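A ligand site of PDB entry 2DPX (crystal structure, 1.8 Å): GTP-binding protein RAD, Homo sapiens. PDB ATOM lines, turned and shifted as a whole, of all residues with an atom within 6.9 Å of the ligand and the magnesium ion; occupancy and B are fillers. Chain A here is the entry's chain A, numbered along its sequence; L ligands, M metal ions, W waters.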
ATOM      1  N   GLY A  14     -22.262  36.758  17.859  1.00  0.00           N
ATOM      2  CA  GLY A  14     -21.957  35.470  17.273  1.00  0.00           C
ATOM      3  C   GLY A  14     -21.933  35.444  15.757  1.00  0.00           C
ATOM      4  O   GLY A  14     -22.479  36.334  15.099  1.00  0.00           O
ATOM      5  N   ALA A  15     -21.286  34.420  15.201  1.00  0.00           N
ATOM      6  CA  ALA A  15     -21.210  34.243  13.769  1.00  0.00           C
ATOM      7  C   ALA A  15     -22.606  34.034  13.179  1.00  0.00           C
ATOM      8  O   ALA A  15     -23.552  33.625  13.876  1.00  0.00           O
ATOM      9  CB  ALA A  15     -20.322  33.034  13.435  1.00  0.00           C
ATOM     10  N   PRO A  16     -22.769  34.301  11.881  1.00  0.00           N
ATOM     11  CA  PRO A  16     -24.084  34.107  11.276  1.00  0.00           C
ATOM     12  C   PRO A  16     -24.471  32.640  11.272  1.00  0.00           C
ATOM     13  O   PRO A  16     -23.622  31.753  11.213  1.00  0.00           O
ATOM     14  CB  PRO A  16     -23.905  34.677   9.863  1.00  0.00           C
ATOM     15  CG  PRO A  16     -22.448  34.436   9.582  1.00  0.00           C
ATOM     16  CD  PRO A  16     -21.793  34.799  10.892  1.00  0.00           C
ATOM     17  N   GLY A  17     -25.774  32.390  11.375  1.00  0.00           N
ATOM     18  CA  GLY A  17     -26.284  31.040  11.337  1.00  0.00           C
ATOM     19  C   GLY A  17     -26.239  30.237  12.631  1.00  0.00           C
ATOM     20  O   GLY A  17     -26.616  29.054  12.611  1.00  0.00           O
ATOM     21  N   VAL A  18     -25.822  30.849  13.742  1.00  0.00           N
ATOM     22  CA  VAL A  18     -25.736  30.095  14.999  1.00  0.00           C
ATOM     23  C   VAL A  18     -26.999  30.001  15.856  1.00  0.00           C
ATOM     24  O   VAL A  18     -27.080  29.170  16.774  1.00  0.00           O
ATOM     25  CB  VAL A  18     -24.558  30.596  15.887  1.00  0.00           C
ATOM     26  CG1 VAL A  18     -23.273  30.613  15.083  1.00  0.00           C
ATOM     27  CG2 VAL A  18     -24.856  31.991  16.446  1.00  0.00           C
ATOM     28  N   GLY A  19     -27.988  30.843  15.552  1.00  0.00           N
ATOM     29  CA  GLY A  19     -29.226  30.814  16.300  1.00  0.00           C
ATOM     30  C   GLY A  19     -29.498  32.023  17.180  1.00  0.00           C
ATOM     31  O   GLY A  19     -30.342  31.966  18.066  1.00  0.00           O
ATOM     32  N   LYS A  20     -28.786  33.122  16.943  1.00  0.00           N
ATOM     33  CA  LYS A  20     -29.021  34.299  17.771  1.00  0.00           C
ATOM     34  C   LYS A  20     -30.466  34.760  17.652  1.00  0.00           C
ATOM     35  O   LYS A  20     -31.147  34.973  18.658  1.00  0.00           O
ATOM     36  CB  LYS A  20     -28.083  35.446  17.338  1.00  0.00           C
ATOM     37  CG  LYS A  20     -26.578  35.131  17.473  1.00  0.00           C
ATOM     38  CD  LYS A  20     -25.662  36.325  17.105  1.00  0.00           C
ATOM     39  CE  LYS A  20     -25.848  36.755  15.649  1.00  0.00           C
ATOM     40  NZ  LYS A  20     -25.578  35.709  14.609  1.00  0.00           N
ATOM     41  N   SER A  21     -30.938  34.922  16.429  1.00  0.00           N
ATOM     42  CA  SER A  21     -32.306  35.381  16.229  1.00  0.00           C
ATOM     43  C   SER A  21     -33.299  34.357  16.751  1.00  0.00           C
ATOM     44  O   SER A  21     -34.317  34.709  17.333  1.00  0.00           O
ATOM     45  CB  SER A  21     -32.533  35.688  14.756  1.00  0.00           C
ATOM     46  OG  SER A  21     -31.669  36.739  14.351  1.00  0.00           O
ATOM     47  N   ALA A  22     -32.984  33.075  16.566  1.00  0.00           N
ATOM     48  CA  ALA A  22     -33.890  32.022  17.047  1.00  0.00           C
ATOM     49  C   ALA A  22     -34.058  32.147  18.562  1.00  0.00           C
ATOM     50  O   ALA A  22     -35.175  32.050  19.089  1.00  0.00           O
ATOM     51  CB  ALA A  22     -33.322  30.652  16.674  1.00  0.00           C
ATOM     52  N   LEU A  23     -32.952  32.364  19.272  1.00  0.00           N
ATOM     53  CA  LEU A  23     -32.979  32.507  20.728  1.00  0.00           C
ATOM     54  C   LEU A  23     -33.653  33.791  21.179  1.00  0.00           C
ATOM     55  O   LEU A  23     -34.382  33.792  22.165  1.00  0.00           O
ATOM     56  CB  LEU A  23     -31.555  32.475  21.310  1.00  0.00           C
ATOM     57  CG  LEU A  23     -30.763  31.179  21.189  1.00  0.00           C
ATOM     58  CD1 LEU A  23     -29.322  31.416  21.578  1.00  0.00           C
ATOM     59  CD2 LEU A  23     -31.386  30.118  22.098  1.00  0.00           C
ATOM     60  N   ARG A  25     -36.049  35.494  19.615  1.00  0.00           N
ATOM     61  CA  ARG A  25     -37.505  35.439  19.358  1.00  0.00           C
ATOM     62  C   ARG A  25     -38.231  34.581  20.372  1.00  0.00           C
ATOM     63  O   ARG A  25     -39.354  34.895  20.768  1.00  0.00           O
ATOM     64  CB  ARG A  25     -37.771  34.941  17.943  1.00  0.00           C
ATOM     65  CG  ARG A  25     -37.303  35.905  16.859  1.00  0.00           C
ATOM     66  CD  ARG A  25     -37.539  35.324  15.480  1.00  0.00           C
ATOM     67  NE  ARG A  25     -37.145  33.915  15.464  1.00  0.00           N
ATOM     68  CZ  ARG A  25     -36.933  33.202  14.370  1.00  0.00           C
ATOM     69  NH1 ARG A  25     -37.054  33.752  13.166  1.00  0.00           N
ATOM     70  NH2 ARG A  25     -36.577  31.929  14.482  1.00  0.00           N
ATOM     71  N   ASP A  60     -30.747  42.060  19.211  1.00  0.00           N
ATOM     72  CA  ASP A  60     -30.296  41.070  18.268  1.00  0.00           C
ATOM     73  C   ASP A  60     -29.855  41.869  17.039  1.00  0.00           C
ATOM     74  O   ASP A  60     -30.449  41.761  15.972  1.00  0.00           O
ATOM     75  CB  ASP A  60     -31.450  40.148  17.923  1.00  0.00           C
ATOM     76  CG  ASP A  60     -31.080  39.117  16.901  1.00  0.00           C
ATOM     77  OD1 ASP A  60     -29.878  38.787  16.795  1.00  0.00           O
ATOM     78  OD2 ASP A  60     -31.985  38.628  16.193  1.00  0.00           O
ATOM     79  N   TRP A  62     -26.255  42.218  16.054  1.00  0.00           N
ATOM     80  CA  TRP A  62     -24.906  41.941  15.596  1.00  0.00           C
ATOM     81  C   TRP A  62     -24.882  41.642  14.096  1.00  0.00           C
ATOM     82  O   TRP A  62     -25.606  40.767  13.616  1.00  0.00           O
ATOM     83  CB  TRP A  62     -24.329  40.760  16.361  1.00  0.00           C
ATOM     84  CG  TRP A  62     -22.910  40.505  16.045  1.00  0.00           C
ATOM     85  CD1 TRP A  62     -22.410  39.441  15.355  1.00  0.00           C
ATOM     86  CD2 TRP A  62     -21.799  41.324  16.399  1.00  0.00           C
ATOM     87  NE1 TRP A  62     -21.044  39.542  15.258  1.00  0.00           N
ATOM     88  CE2 TRP A  62     -20.634  40.691  15.904  1.00  0.00           C
ATOM     89  CE3 TRP A  62     -21.654  42.526  17.113  1.00  0.00           C
ATOM     90  CZ2 TRP A  62     -19.350  41.218  16.069  1.00  0.00           C
ATOM     91  CZ3 TRP A  62     -20.382  43.055  17.282  1.00  0.00           C
ATOM     92  CH2 TRP A  62     -19.250  42.395  16.771  1.00  0.00           C
ATOM     93  N   VAL A  84     -22.754  33.584  21.330  1.00  0.00           N
ATOM     94  CA  VAL A  84     -23.361  32.343  20.851  1.00  0.00           C
ATOM     95  C   VAL A  84     -22.585  31.681  19.718  1.00  0.00           C
ATOM     96  O   VAL A  84     -22.142  32.354  18.798  1.00  0.00           O
ATOM     97  CB  VAL A  84     -24.807  32.591  20.301  1.00  0.00           C
ATOM     98  CG1 VAL A  84     -25.442  31.242  19.876  1.00  0.00           C
ATOM     99  CG2 VAL A  84     -25.675  33.297  21.351  1.00  0.00           C
ATOM    100  N   ASN A 119     -25.251  26.641  21.056  1.00  0.00           N
ATOM    101  CA  ASN A 119     -26.608  26.332  20.594  1.00  0.00           C
ATOM    102  C   ASN A 119     -26.698  25.158  19.626  1.00  0.00           C
ATOM    103  O   ASN A 119     -25.680  24.693  19.113  1.00  0.00           O
ATOM    104  CB  ASN A 119     -27.215  27.614  19.974  1.00  0.00           C
ATOM    105  CG  ASN A 119     -28.695  27.486  19.641  1.00  0.00           C
ATOM    106  OD1 ASN A 119     -29.488  26.970  20.429  1.00  0.00           O
ATOM    107  ND2 ASN A 119     -29.081  27.986  18.463  1.00  0.00           N
ATOM    108  N   LYS A 120     -27.934  24.683  19.404  1.00  0.00           N
ATOM    109  CA  LYS A 120     -28.256  23.562  18.506  1.00  0.00           C
ATOM    110  C   LYS A 120     -27.907  22.197  19.121  1.00  0.00           C
ATOM    111  O   LYS A 120     -27.523  21.273  18.426  1.00  0.00           O
ATOM    112  CB  LYS A 120     -27.541  23.728  17.152  1.00  0.00           C
ATOM    113  CG  LYS A 120     -27.845  25.083  16.457  1.00  0.00           C
ATOM    114  CD  LYS A 120     -27.520  25.056  14.952  1.00  0.00           C
ATOM    115  CE  LYS A 120     -27.824  26.401  14.261  1.00  0.00           C
ATOM    116  NZ  LYS A 120     -27.466  26.363  12.811  1.00  0.00           N
ATOM    117  N   SER A 121     -28.039  22.084  20.443  1.00  0.00           N
ATOM    118  CA  SER A 121     -27.716  20.826  21.109  1.00  0.00           C
ATOM    119  C   SER A 121     -28.580  19.651  20.625  1.00  0.00           C
ATOM    120  O   SER A 121     -28.237  18.501  20.858  1.00  0.00           O
ATOM    121  CB  SER A 121     -27.892  20.977  22.609  1.00  0.00           C
ATOM    122  OG  SER A 121     -29.234  21.296  22.900  1.00  0.00           O
ATOM    123  N   ASP A 122     -29.698  19.951  19.948  1.00  0.00           N
ATOM    124  CA  ASP A 122     -30.569  18.895  19.437  1.00  0.00           C
ATOM    125  C   ASP A 122     -29.996  18.168  18.211  1.00  0.00           C
ATOM    126  O   ASP A 122     -30.402  17.049  17.918  1.00  0.00           O
ATOM    127  CB  ASP A 122     -31.942  19.473  19.047  1.00  0.00           C
ATOM    128  CG  ASP A 122     -31.838  20.596  18.024  1.00  0.00           C
ATOM    129  OD1 ASP A 122     -31.223  21.643  18.337  1.00  0.00           O
ATOM    130  OD2 ASP A 122     -32.361  20.434  16.906  1.00  0.00           O
ATOM    131  N   LEU A 123     -29.079  18.809  17.502  1.00  0.00           N
ATOM    132  CA  LEU A 123     -28.492  18.200  16.305  1.00  0.00           C
ATOM    133  C   LEU A 123     -27.294  17.333  16.718  1.00  0.00           C
ATOM    134  O   LEU A 123     -26.134  17.616  16.394  1.00  0.00           O
ATOM    135  CB  LEU A 123     -28.069  19.305  15.333  1.00  0.00           C
ATOM    136  CG  LEU A 123     -29.174  20.251  14.850  1.00  0.00           C
ATOM    137  CD1 LEU A 123     -28.591  21.282  13.887  1.00  0.00           C
ATOM    138  CD2 LEU A 123     -30.289  19.467  14.174  1.00  0.00           C
ATOM    139  N   THR A 148     -27.747  25.236  24.622  1.00  0.00           N
ATOM    140  CA  THR A 148     -29.152  25.408  24.344  1.00  0.00           C
ATOM    141  C   THR A 148     -29.587  24.748  23.056  1.00  0.00           C
ATOM    142  O   THR A 148     -28.776  24.306  22.238  1.00  0.00           O
ATOM    143  CB  THR A 148     -29.488  26.899  24.189  1.00  0.00           C
ATOM    144  OG1 THR A 148     -28.707  27.446  23.125  1.00  0.00           O
ATOM    145  CG2 THR A 148     -29.179  27.680  25.452  1.00  0.00           C
ATOM    146  N   SER A 149     -30.905  24.683  22.890  1.00  0.00           N
ATOM    147  CA  SER A 149     -31.497  24.197  21.682  1.00  0.00           C
ATOM    148  C   SER A 149     -32.700  25.105  21.427  1.00  0.00           C
ATOM    149  O   SER A 149     -33.711  25.008  22.121  1.00  0.00           O
ATOM    150  CB  SER A 149     -32.011  22.755  21.820  1.00  0.00           C
ATOM    151  OG  SER A 149     -32.769  22.462  20.657  1.00  0.00           O
ATOM    152  N   ALA A 150     -32.562  25.999  20.453  1.00  0.00           N
ATOM    153  CA  ALA A 150     -33.675  26.885  20.119  1.00  0.00           C
ATOM    154  C   ALA A 150     -34.772  26.047  19.497  1.00  0.00           C
ATOM    155  O   ALA A 150     -35.958  26.391  19.558  1.00  0.00           O
ATOM    156  CB  ALA A 150     -33.227  27.968  19.120  1.00  0.00           C
ATOM    157  N   ALA A 151     -34.391  24.937  18.875  1.00  0.00           N
ATOM    158  CA  ALA A 151     -35.385  24.075  18.252  1.00  0.00           C
ATOM    159  C   ALA A 151     -36.340  23.455  19.288  1.00  0.00           C
ATOM    160  O   ALA A 151     -37.545  23.366  19.067  1.00  0.00           O
ATOM    161  CB  ALA A 151     -34.694  22.967  17.457  1.00  0.00           C
ATOM    162  N   LEU A 152     -35.783  23.031  20.421  1.00  0.00           N
ATOM    163  CA  LEU A 152     -36.581  22.405  21.474  1.00  0.00           C
ATOM    164  C   LEU A 152     -36.899  23.351  22.613  1.00  0.00           C
ATOM    165  O   LEU A 152     -37.545  22.950  23.588  1.00  0.00           O
ATOM    166  CB  LEU A 152     -35.820  21.214  22.058  1.00  0.00           C
ATOM    167  CG  LEU A 152     -35.398  20.175  21.017  1.00  0.00           C
ATOM    168  CD1 LEU A 152     -34.664  18.988  21.693  1.00  0.00           C
ATOM    169  CD2 LEU A 152     -36.639  19.690  20.304  1.00  0.00           C
ATOM    170  N   HIS A 153     -36.467  24.601  22.502  1.00  0.00           N
ATOM    171  CA  HIS A 153     -36.657  25.558  23.591  1.00  0.00           C
ATOM    172  C   HIS A 153     -35.917  25.067  24.860  1.00  0.00           C
ATOM    173  O   HIS A 153     -36.265  25.447  25.978  1.00  0.00           O
ATOM    174  CB  HIS A 153     -38.150  25.756  23.896  1.00  0.00           C
ATOM    175  CG  HIS A 153     -38.900  26.498  22.827  1.00  0.00           C
ATOM    176  ND1 HIS A 153     -38.440  26.596  21.535  1.00  0.00           N
ATOM    177  CD2 HIS A 153     -40.070  27.178  22.866  1.00  0.00           C
ATOM    178  CE1 HIS A 153     -39.295  27.306  20.817  1.00  0.00           C
ATOM    179  NE2 HIS A 153     -40.290  27.664  21.606  1.00  0.00           N
HETATM  180  P1  LIG L   1     -28.538  33.829  13.419  1.00  0.00           P
HETATM  181  O1  LIG L   1     -28.006  34.117  12.096  1.00  0.00           O
HETATM  182  O2  LIG L   1     -27.390  33.679  14.425  1.00  0.00           O
HETATM  183  O3  LIG L   1     -29.481  34.841  13.877  1.00  0.00           O
HETATM  184  O4  LIG L   1     -29.252  32.387  13.382  1.00  0.00           O
HETATM  185  P2  LIG L   1     -30.789  32.102  13.002  1.00  0.00           P
HETATM  186  O5  LIG L   1     -31.678  32.317  14.169  1.00  0.00           O
HETATM  187  O6  LIG L   1     -31.214  32.956  11.794  1.00  0.00           O
HETATM  188  O7  LIG L   1     -30.845  30.573  12.638  1.00  0.00           O
HETATM  189  C1  LIG L   1     -29.902  30.045  11.716  1.00  0.00           C
HETATM  190  C2  LIG L   1     -30.329  28.627  11.287  1.00  0.00           C
HETATM  191  O8  LIG L   1     -30.097  27.689  12.357  1.00  0.00           O
HETATM  192  C3  LIG L   1     -31.809  28.508  10.949  1.00  0.00           C
HETATM  193  O9  LIG L   1     -31.843  27.588   9.835  1.00  0.00           O
HETATM  194  C4  LIG L   1     -32.457  28.021  12.227  1.00  0.00           C
HETATM  195  O10 LIG L   1     -33.659  27.291  11.959  1.00  0.00           O
HETATM  196  C5  LIG L   1     -31.372  27.102  12.749  1.00  0.00           C
HETATM  197  N1  LIG L   1     -31.337  26.973  14.202  1.00  0.00           N
HETATM  198  C6  LIG L   1     -31.126  27.965  15.124  1.00  0.00           C
HETATM  199  N2  LIG L   1     -31.108  27.431  16.390  1.00  0.00           N
HETATM  200  C7  LIG L   1     -31.310  26.094  16.233  1.00  0.00           C
HETATM  201  C8  LIG L   1     -31.384  24.947  17.139  1.00  0.00           C
HETATM  202  O11 LIG L   1     -31.245  25.125  18.365  1.00  0.00           O
HETATM  203  N3  LIG L   1     -31.617  23.689  16.607  1.00  0.00           N
HETATM  204  C9  LIG L   1     -31.762  23.518  15.234  1.00  0.00           C
HETATM  205  N4  LIG L   1     -31.998  22.308  14.717  1.00  0.00           N
HETATM  206  N5  LIG L   1     -31.681  24.564  14.372  1.00  0.00           N
HETATM  207  C10 LIG L   1     -31.459  25.824  14.828  1.00  0.00           C
HETATM  208 MG    MG M   1     -30.203  36.649  13.087  1.00  0.00          MG
HETATM  209  O   HOH W   1     -34.197  31.589  13.415  1.00  0.00           O
HETATM  210  O   HOH W   2     -29.017  37.800  14.235  1.00  0.00           O
HETATM  211  O   HOH W   3     -29.377  24.304  11.947  1.00  0.00           O
HETATM  212  O   HOH W   4     -35.330  28.280   9.646  1.00  0.00           O
HETATM  213  O   HOH W   5     -28.745  36.492  11.681  1.00  0.00           O
HETATM  214  O   HOH W   6     -35.134  28.684  13.719  1.00  0.00           O
HETATM  215  O   HOH W   7     -30.904  38.431  11.988  1.00  0.00           O
HETATM  216  O   HOH W   8     -30.164  25.072   9.547  1.00  0.00           O
HETATM  217  O   HOH W   9     -31.319  35.599  11.707  1.00  0.00           O
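The backbone NH of Gly 19 is in hydrogen-bond range of an oxygen (O4) of the ligand (2.9 Å).
N of Lys 120 sits close to O11 of the ligand (3.5 Å).
N2 of the ligand sits at hydrogen-bond distance from ND2 of Asn 119 (3.0 Å).
OD1 of Asp 122 is in hydrogen-bond range of N3 of the ligand (2.7 Å).
An oxygen (O8) of the ligand sits at hydrogen-bond distance from the side-chain amino group of Lys 120 (3.0 Å).
N of Ala 22 sits at hydrogen-bond distance from O5 of the ligand, at 2.8 Å.
N of Ser 21 sits close to O3 of the ligand.
O11 of the ligand is in hydrogen-bond range of N of Ala 151 (3.2 Å).
The backbone NH of Val 18 is in hydrogen-bond range of an oxygen (O2) of the ligand (3.3 Å).
N of Ala 150 is in hydrogen-bond range of O11 of the ligand (2.6 Å).
O2 of the ligand lies within salt-bridge range of NZ of Lys 20, 2.7 Å away.
The backbone NH (N) of Lys 20 lies within hydrogen-bond range of an oxygen (O2) of the ligand (2.9 Å).
O1 of the ligand lies within hydrogen-bond range of N of Gly 17 (2.9 Å).
The backbone carbonyl oxygen of Ala 150 sits at hydrogen-bond distance from a ring nitrogen (ND1) of His 153, at 3.2 Å.
The backbone carbonyl oxygen (O) of Ala 15 sits at hydrogen-bond distance from the side-chain amino group (NZ) of Lys 20 (3.0 Å).
The side-chain hydroxyl of Ser 149 sits close to the backbone NH of Ala 151, 3.5 Å away.
The backbone NH of Lys 120 sits at hydrogen-bond distance from the backbone carbonyl oxygen of Thr 148 (3.0 Å).
OD1 of Asp 122 lies within hydrogen-bond range of OG of Ser 149 (2.9 Å).
NZ of Lys 120 lies within hydrogen-bond range of O of Gly 17.
The backbone carbonyl oxygen of Val 18 is in hydrogen-bond range of the side-chain amide nitrogen of Asn 119 (2.9 Å).
The guanidinium group (NE) of Arg 25 lies close to the backbone carbonyl oxygen (O) of Ser 21, at 3.5 Å.
Residues that only touch the ligand: Ala 15 (3.9 Å), Pro 16 (3.9 Å), Leu 123 (3.4 Å) and Ser 149 (3.4 Å).
Within 4 Å of the ligand: Ala 15, Pro 16, Gly 17, Val 18, Gly 19, Lys 20, Ser 21, Ala 22, Asn 119, Lys 120, Asp 122, Leu 123, Ser 149, Ala 150 and Ala 151.
Within 4 Å of the magnesium ion: Ser 21.
The nearest printed residue that does not touch the magnesium ion is Asp 60 (4.1 Å).
The magnesium ion is bound by OG of Ser 21 (1.9 Å), water W2 (2.0 Å), water W5 (2.0 Å), water W9 (2.1 Å), O3 of the ligand (2.1 Å) and water W7 (2.2 Å).
Water W1 lies within hydrogen-bond range of NH2 of Arg 25 and O5 of the ligand.
Water W3 bridges NZ of Lys 120 and N5 of the ligand.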
